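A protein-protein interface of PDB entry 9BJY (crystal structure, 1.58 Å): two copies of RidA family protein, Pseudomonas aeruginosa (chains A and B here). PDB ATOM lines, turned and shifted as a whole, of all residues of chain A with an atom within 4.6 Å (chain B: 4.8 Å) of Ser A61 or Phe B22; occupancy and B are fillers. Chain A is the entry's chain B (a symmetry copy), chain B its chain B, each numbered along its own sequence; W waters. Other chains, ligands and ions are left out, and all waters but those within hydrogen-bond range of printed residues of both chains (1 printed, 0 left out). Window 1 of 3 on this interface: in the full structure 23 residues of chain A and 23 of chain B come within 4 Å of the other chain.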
ATOM      1  N   ILE A  59      18.283 -14.650  -7.685  1.00  0.00           N
ATOM      2  CA  ILE A  59      19.055 -15.885  -7.620  1.00  0.00           C
ATOM      3  C   ILE A  59      20.529 -15.556  -7.805  1.00  0.00           C
ATOM      4  O   ILE A  59      20.905 -14.763  -8.687  1.00  0.00           O
ATOM      5  CB  ILE A  59      18.548 -16.909  -8.653  1.00  0.00           C
ATOM      6  CG1 ILE A  59      17.093 -17.254  -8.347  1.00  0.00           C
ATOM      7  CG2 ILE A  59      19.432 -18.168  -8.615  1.00  0.00           C
ATOM      8  CD1 ILE A  59      16.349 -18.062  -9.432  1.00  0.00           C
ATOM      9  N   LEU A  60      21.375 -16.162  -6.962  1.00  0.00           N
ATOM     10  CA  LEU A  60      22.822 -15.982  -7.011  1.00  0.00           C
ATOM     11  C   LEU A  60      23.512 -17.107  -7.766  1.00  0.00           C
ATOM     12  O   LEU A  60      24.383 -16.842  -8.604  1.00  0.00           O
ATOM     13  CB  LEU A  60      23.391 -15.864  -5.595  1.00  0.00           C
ATOM     14  CG  LEU A  60      22.734 -14.717  -4.795  1.00  0.00           C
ATOM     15  CD1 LEU A  60      23.206 -14.772  -3.335  1.00  0.00           C
ATOM     16  CD2 LEU A  60      22.969 -13.357  -5.435  1.00  0.00           C
ATOM     17  N   SER A  61      23.107 -18.350  -7.519  1.00  0.00           N
ATOM     18  CA  SER A  61      23.750 -19.493  -8.146  1.00  0.00           C
ATOM     19  C   SER A  61      22.728 -20.601  -8.317  1.00  0.00           C
ATOM     20  O   SER A  61      21.808 -20.752  -7.508  1.00  0.00           O
ATOM     21  CB  SER A  61      24.933 -19.993  -7.308  1.00  0.00           C
ATOM     22  OG  SER A  61      24.484 -20.437  -6.030  1.00  0.00           O
ATOM     23  N   ALA A  62      22.927 -21.411  -9.360  1.00  0.00           N
ATOM     24  CA  ALA A  62      22.120 -22.589  -9.578  1.00  0.00           C
ATOM     25  C   ALA A  62      23.013 -23.710 -10.095  1.00  0.00           C
ATOM     26  O   ALA A  62      23.716 -23.515 -11.091  1.00  0.00           O
ATOM     27  CB  ALA A  62      21.030 -22.303 -10.619  1.00  0.00           C
ATOM     28  N   THR A  63      23.002 -24.864  -9.425  1.00  0.00           N
ATOM     29  CA  THR A  63      23.595 -26.074  -9.983  1.00  0.00           C
ATOM     30  C   THR A  63      22.449 -26.848 -10.592  1.00  0.00           C
ATOM     31  O   THR A  63      21.490 -27.172  -9.886  1.00  0.00           O
ATOM     32  CB  THR A  63      24.316 -26.962  -8.979  1.00  0.00           C
ATOM     33  OG1 THR A  63      25.320 -26.197  -8.320  1.00  0.00           O
ATOM     34  CG2 THR A  63      24.985 -28.163  -9.707  1.00  0.00           C
ATOM     35  N   PRO A  90      21.305 -15.878 -13.285  1.00  0.00           N
ATOM     36  CA  PRO A  90      22.247 -16.085 -12.193  1.00  0.00           C
ATOM     37  C   PRO A  90      23.524 -16.763 -12.690  1.00  0.00           C
ATOM     38  O   PRO A  90      23.655 -17.129 -13.856  1.00  0.00           O
ATOM     39  CB  PRO A  90      21.474 -17.010 -11.252  1.00  0.00           C
ATOM     40  CG  PRO A  90      20.734 -17.901 -12.217  1.00  0.00           C
ATOM     41  CD  PRO A  90      20.269 -16.946 -13.312  1.00  0.00           C
ATOM     42  N   SER A  91      24.482 -16.934 -11.786  1.00  0.00           N
ATOM     43  CA  SER A  91      25.560 -17.869 -12.092  1.00  0.00           C
ATOM     44  C   SER A  91      24.980 -19.281 -12.141  1.00  0.00           C
ATOM     45  O   SER A  91      24.014 -19.603 -11.442  1.00  0.00           O
ATOM     46  CB  SER A  91      26.692 -17.760 -11.081  1.00  0.00           C
ATOM     47  OG  SER A  91      26.376 -18.297  -9.806  1.00  0.00           O
ATOM     48  N   THR A 109      19.560 -26.859  -7.727  1.00  0.00           N
ATOM     49  CA  THR A 109      19.892 -26.382  -6.383  1.00  0.00           C
ATOM     50  C   THR A 109      20.290 -24.913  -6.440  1.00  0.00           C
ATOM     51  O   THR A 109      21.261 -24.565  -7.120  1.00  0.00           O
ATOM     52  CB  THR A 109      21.028 -27.211  -5.800  1.00  0.00           C
ATOM     53  OG1 THR A 109      20.672 -28.585  -5.786  1.00  0.00           O
ATOM     54  CG2 THR A 109      21.376 -26.718  -4.405  1.00  0.00           C
ATOM     55  N   VAL A 110      19.554 -24.060  -5.709  1.00  0.00           N
ATOM     56  CA  VAL A 110      19.648 -22.614  -5.808  1.00  0.00           C
ATOM     57  C   VAL A 110      20.120 -22.017  -4.494  1.00  0.00           C
ATOM     58  O   VAL A 110      19.718 -22.466  -3.419  1.00  0.00           O
ATOM     59  CB  VAL A 110      18.268 -22.024  -6.200  1.00  0.00           C
ATOM     60  CG1 VAL A 110      18.135 -20.544  -5.817  1.00  0.00           C
ATOM     61  CG2 VAL A 110      18.060 -22.232  -7.673  1.00  0.00           C
ATOM     62  N   VAL A 111      20.966 -20.992  -4.594  1.00  0.00           N
ATOM     63  CA  VAL A 111      21.230 -20.053  -3.509  1.00  0.00           C
ATOM     64  C   VAL A 111      20.785 -18.691  -4.015  1.00  0.00           C
ATOM     65  O   VAL A 111      21.063 -18.334  -5.167  1.00  0.00           O
ATOM     66  CB  VAL A 111      22.717 -20.029  -3.093  1.00  0.00           C
ATOM     67  CG1 VAL A 111      22.966 -19.066  -1.927  1.00  0.00           C
ATOM     68  CG2 VAL A 111      23.167 -21.419  -2.727  1.00  0.00           C
ATOM     69  N   ALA B  13      28.386 -14.751 -15.909  1.00  0.00           N
ATOM     70  CA  ALA B  13      29.653 -15.379 -15.526  1.00  0.00           C
ATOM     71  C   ALA B  13      29.901 -15.257 -14.026  1.00  0.00           C
ATOM     72  O   ALA B  13      30.472 -16.166 -13.403  1.00  0.00           O
ATOM     73  CB  ALA B  13      30.825 -14.747 -16.291  1.00  0.00           C
ATOM     74  N   ALA B  14      29.513 -14.139 -13.429  1.00  0.00           N
ATOM     75  CA  ALA B  14      29.580 -13.962 -11.989  1.00  0.00           C
ATOM     76  C   ALA B  14      28.386 -13.159 -11.490  1.00  0.00           C
ATOM     77  O   ALA B  14      27.861 -12.283 -12.190  1.00  0.00           O
ATOM     78  CB  ALA B  14      30.875 -13.260 -11.574  1.00  0.00           C
ATOM     79  N   VAL B  15      27.963 -13.468 -10.261  1.00  0.00           N
ATOM     80  CA  VAL B  15      27.003 -12.660  -9.521  1.00  0.00           C
ATOM     81  C   VAL B  15      27.645 -12.286  -8.189  1.00  0.00           C
ATOM     82  O   VAL B  15      28.187 -13.156  -7.492  1.00  0.00           O
ATOM     83  CB  VAL B  15      25.674 -13.399  -9.307  1.00  0.00           C
ATOM     84  CG1 VAL B  15      24.720 -12.519  -8.518  1.00  0.00           C
ATOM     85  CG2 VAL B  15      25.038 -13.777 -10.633  1.00  0.00           C
ATOM     86  N   LEU B  20      30.234 -11.449  -1.284  1.00  0.00           N
ATOM     87  CA  LEU B  20      30.461 -12.746  -1.886  1.00  0.00           C
ATOM     88  C   LEU B  20      30.426 -12.628  -3.409  1.00  0.00           C
ATOM     89  O   LEU B  20      29.696 -11.815  -3.980  1.00  0.00           O
ATOM     90  CB  LEU B  20      29.406 -13.746  -1.440  1.00  0.00           C
ATOM     91  CG  LEU B  20      29.400 -14.106   0.024  1.00  0.00           C
ATOM     92  CD1 LEU B  20      28.198 -14.976   0.314  1.00  0.00           C
ATOM     93  CD2 LEU B  20      30.701 -14.797   0.381  1.00  0.00           C
ATOM     94  N   VAL B  21      31.192 -13.494  -4.061  1.00  0.00           N
ATOM     95  CA  VAL B  21      31.207 -13.623  -5.505  1.00  0.00           C
ATOM     96  C   VAL B  21      30.893 -15.066  -5.864  1.00  0.00           C
ATOM     97  O   VAL B  21      31.601 -15.977  -5.424  1.00  0.00           O
ATOM     98  CB  VAL B  21      32.572 -13.221  -6.078  1.00  0.00           C
ATOM     99  CG1 VAL B  21      32.566 -13.424  -7.559  1.00  0.00           C
ATOM    100  CG2 VAL B  21      32.878 -11.762  -5.723  1.00  0.00           C
ATOM    101  N   PHE B  22      29.882 -15.255  -6.701  1.00  0.00           N
ATOM    102  CA  PHE B  22      29.458 -16.563  -7.185  1.00  0.00           C
ATOM    103  C   PHE B  22      29.814 -16.664  -8.669  1.00  0.00           C
ATOM    104  O   PHE B  22      29.218 -15.974  -9.503  1.00  0.00           O
ATOM    105  CB  PHE B  22      27.945 -16.764  -6.985  1.00  0.00           C
ATOM    106  CG  PHE B  22      27.492 -16.676  -5.553  1.00  0.00           C
ATOM    107  CD1 PHE B  22      27.299 -15.444  -4.938  1.00  0.00           C
ATOM    108  CD2 PHE B  22      27.251 -17.827  -4.814  1.00  0.00           C
ATOM    109  CE1 PHE B  22      26.898 -15.374  -3.620  1.00  0.00           C
ATOM    110  CE2 PHE B  22      26.842 -17.744  -3.484  1.00  0.00           C
ATOM    111  CZ  PHE B  22      26.669 -16.518  -2.901  1.00  0.00           C
ATOM    112  N   LEU B  23      30.750 -17.548  -9.005  1.00  0.00           N
ATOM    113  CA  LEU B  23      31.138 -17.742 -10.394  1.00  0.00           C
ATOM    114  C   LEU B  23      30.408 -18.922 -11.015  1.00  0.00           C
ATOM    115  O   LEU B  23      30.277 -19.988 -10.396  1.00  0.00           O
ATOM    116  CB  LEU B  23      32.640 -17.972 -10.535  1.00  0.00           C
ATOM    117  CG  LEU B  23      33.570 -16.853 -10.083  1.00  0.00           C
ATOM    118  CD1 LEU B  23      35.012 -17.127 -10.505  1.00  0.00           C
ATOM    119  CD2 LEU B  23      33.102 -15.530 -10.587  1.00  0.00           C
ATOM    120  N   SER B  24      29.995 -18.749 -12.263  1.00  0.00           N
ATOM    121  CA  SER B  24      29.522 -19.878 -13.056  1.00  0.00           C
ATOM    122  C   SER B  24      30.641 -20.897 -13.215  1.00  0.00           C
ATOM    123  O   SER B  24      31.824 -20.561 -13.189  1.00  0.00           O
ATOM    124  CB  SER B  24      29.054 -19.393 -14.428  1.00  0.00           C
ATOM    125  OG  SER B  24      27.798 -18.746 -14.342  1.00  0.00           O
ATOM    126  N   VAL B 110      33.360 -21.834  -8.505  1.00  0.00           N
ATOM    127  CA  VAL B 110      34.013 -21.131  -7.414  1.00  0.00           C
ATOM    128  C   VAL B 110      33.049 -20.166  -6.746  1.00  0.00           C
ATOM    129  O   VAL B 110      32.248 -19.511  -7.416  1.00  0.00           O
ATOM    130  CB  VAL B 110      35.250 -20.365  -7.950  1.00  0.00           C
ATOM    131  CG1 VAL B 110      35.670 -19.212  -7.028  1.00  0.00           C
ATOM    132  CG2 VAL B 110      36.371 -21.346  -8.148  1.00  0.00           C
ATOM    133  N   VAL B 111      33.145 -20.076  -5.420  1.00  0.00           N
ATOM    134  CA  VAL B 111      32.605 -18.966  -4.642  1.00  0.00           C
ATOM    135  C   VAL B 111      33.796 -18.308  -3.967  1.00  0.00           C
ATOM    136  O   VAL B 111      34.677 -19.003  -3.444  1.00  0.00           O
ATOM    137  CB  VAL B 111      31.562 -19.424  -3.600  1.00  0.00           C
ATOM    138  CG1 VAL B 111      30.978 -18.238  -2.823  1.00  0.00           C
ATOM    139  CG2 VAL B 111      30.460 -20.191  -4.284  1.00  0.00           C
HETATM  140  O   HOH W   1      28.130 -20.267  -8.893  1.00  0.00           O
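Among the printed residues, pairs that only touch across the chains: Ser A91 with Ser B24 (3.3 Å), Ser A91 with Val B15 (3.4 Å), Ser A91 with Phe B22 (3.5 Å), Leu A60 with Val B15 (3.6 Å), Leu A60 with Phe B22 (3.8 Å), Ser A91 with Leu B23 (3.9 Å), Pro A90 with Val B15 (3.9 Å) and Ser A61 with Phe B22 (3.99 Å).
Hydrophobic or aromatic side chains of chain A that line the printed part of chain B: Leu A60. Of the 10 printed residues of chain B, 4 touch a printed residue of chain A.
Water W1 bridges O of Leu B23 (2.6 Å) and OG of Ser A91 (2.8 Å).
Printed residues of chain A within 4 Å of Phe B22: Leu A60, Ser A61 and Ser A91. Printed residues of chain A within 4 Å of Leu B23: Ser A91 (3.9 Å). Printed residues of chain B within 4 Å of Pro A90: Val B15. Printed residues of chain B within 4 Å of Ser A91: Val B15, Phe B22, Leu B23 and Ser B24. Of the printed residues of chain B, Leu A60 touches Val B15 (3.6 Å) and Phe B22 (3.8 Å). Val B111 touches none of the printed residues of chain A. The nearest printed residue of chain B that does not touch Ser A61 is Val B15 (5.9 Å). The nearest printed residue of chain A that does not touch Leu B23 is Ser A61 (6.2 Å).
Positions printed for both chains: 110 and 111.
O of Ala B13 sits at hydrogen-bond distance from N of Ser B24, at 2.9 Å. The backbone carbonyl oxygen (O) of Val B15 lies within hydrogen-bond range of the backbone NH (N) of Phe B22. OG of Ser A91 sits at hydrogen-bond distance from O of Leu A60 (2.7 Å). The backbone carbonyl oxygen of Val A111 lies within hydrogen-bond range of the backbone NH of Leu A60 (2.8 Å). O of Ser A61 lies within hydrogen-bond range of N of Val A111 (3.0 Å). The backbone NH of Ala A62 sits at hydrogen-bond distance from the backbone carbonyl oxygen of Ser A91 (3.0 Å).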
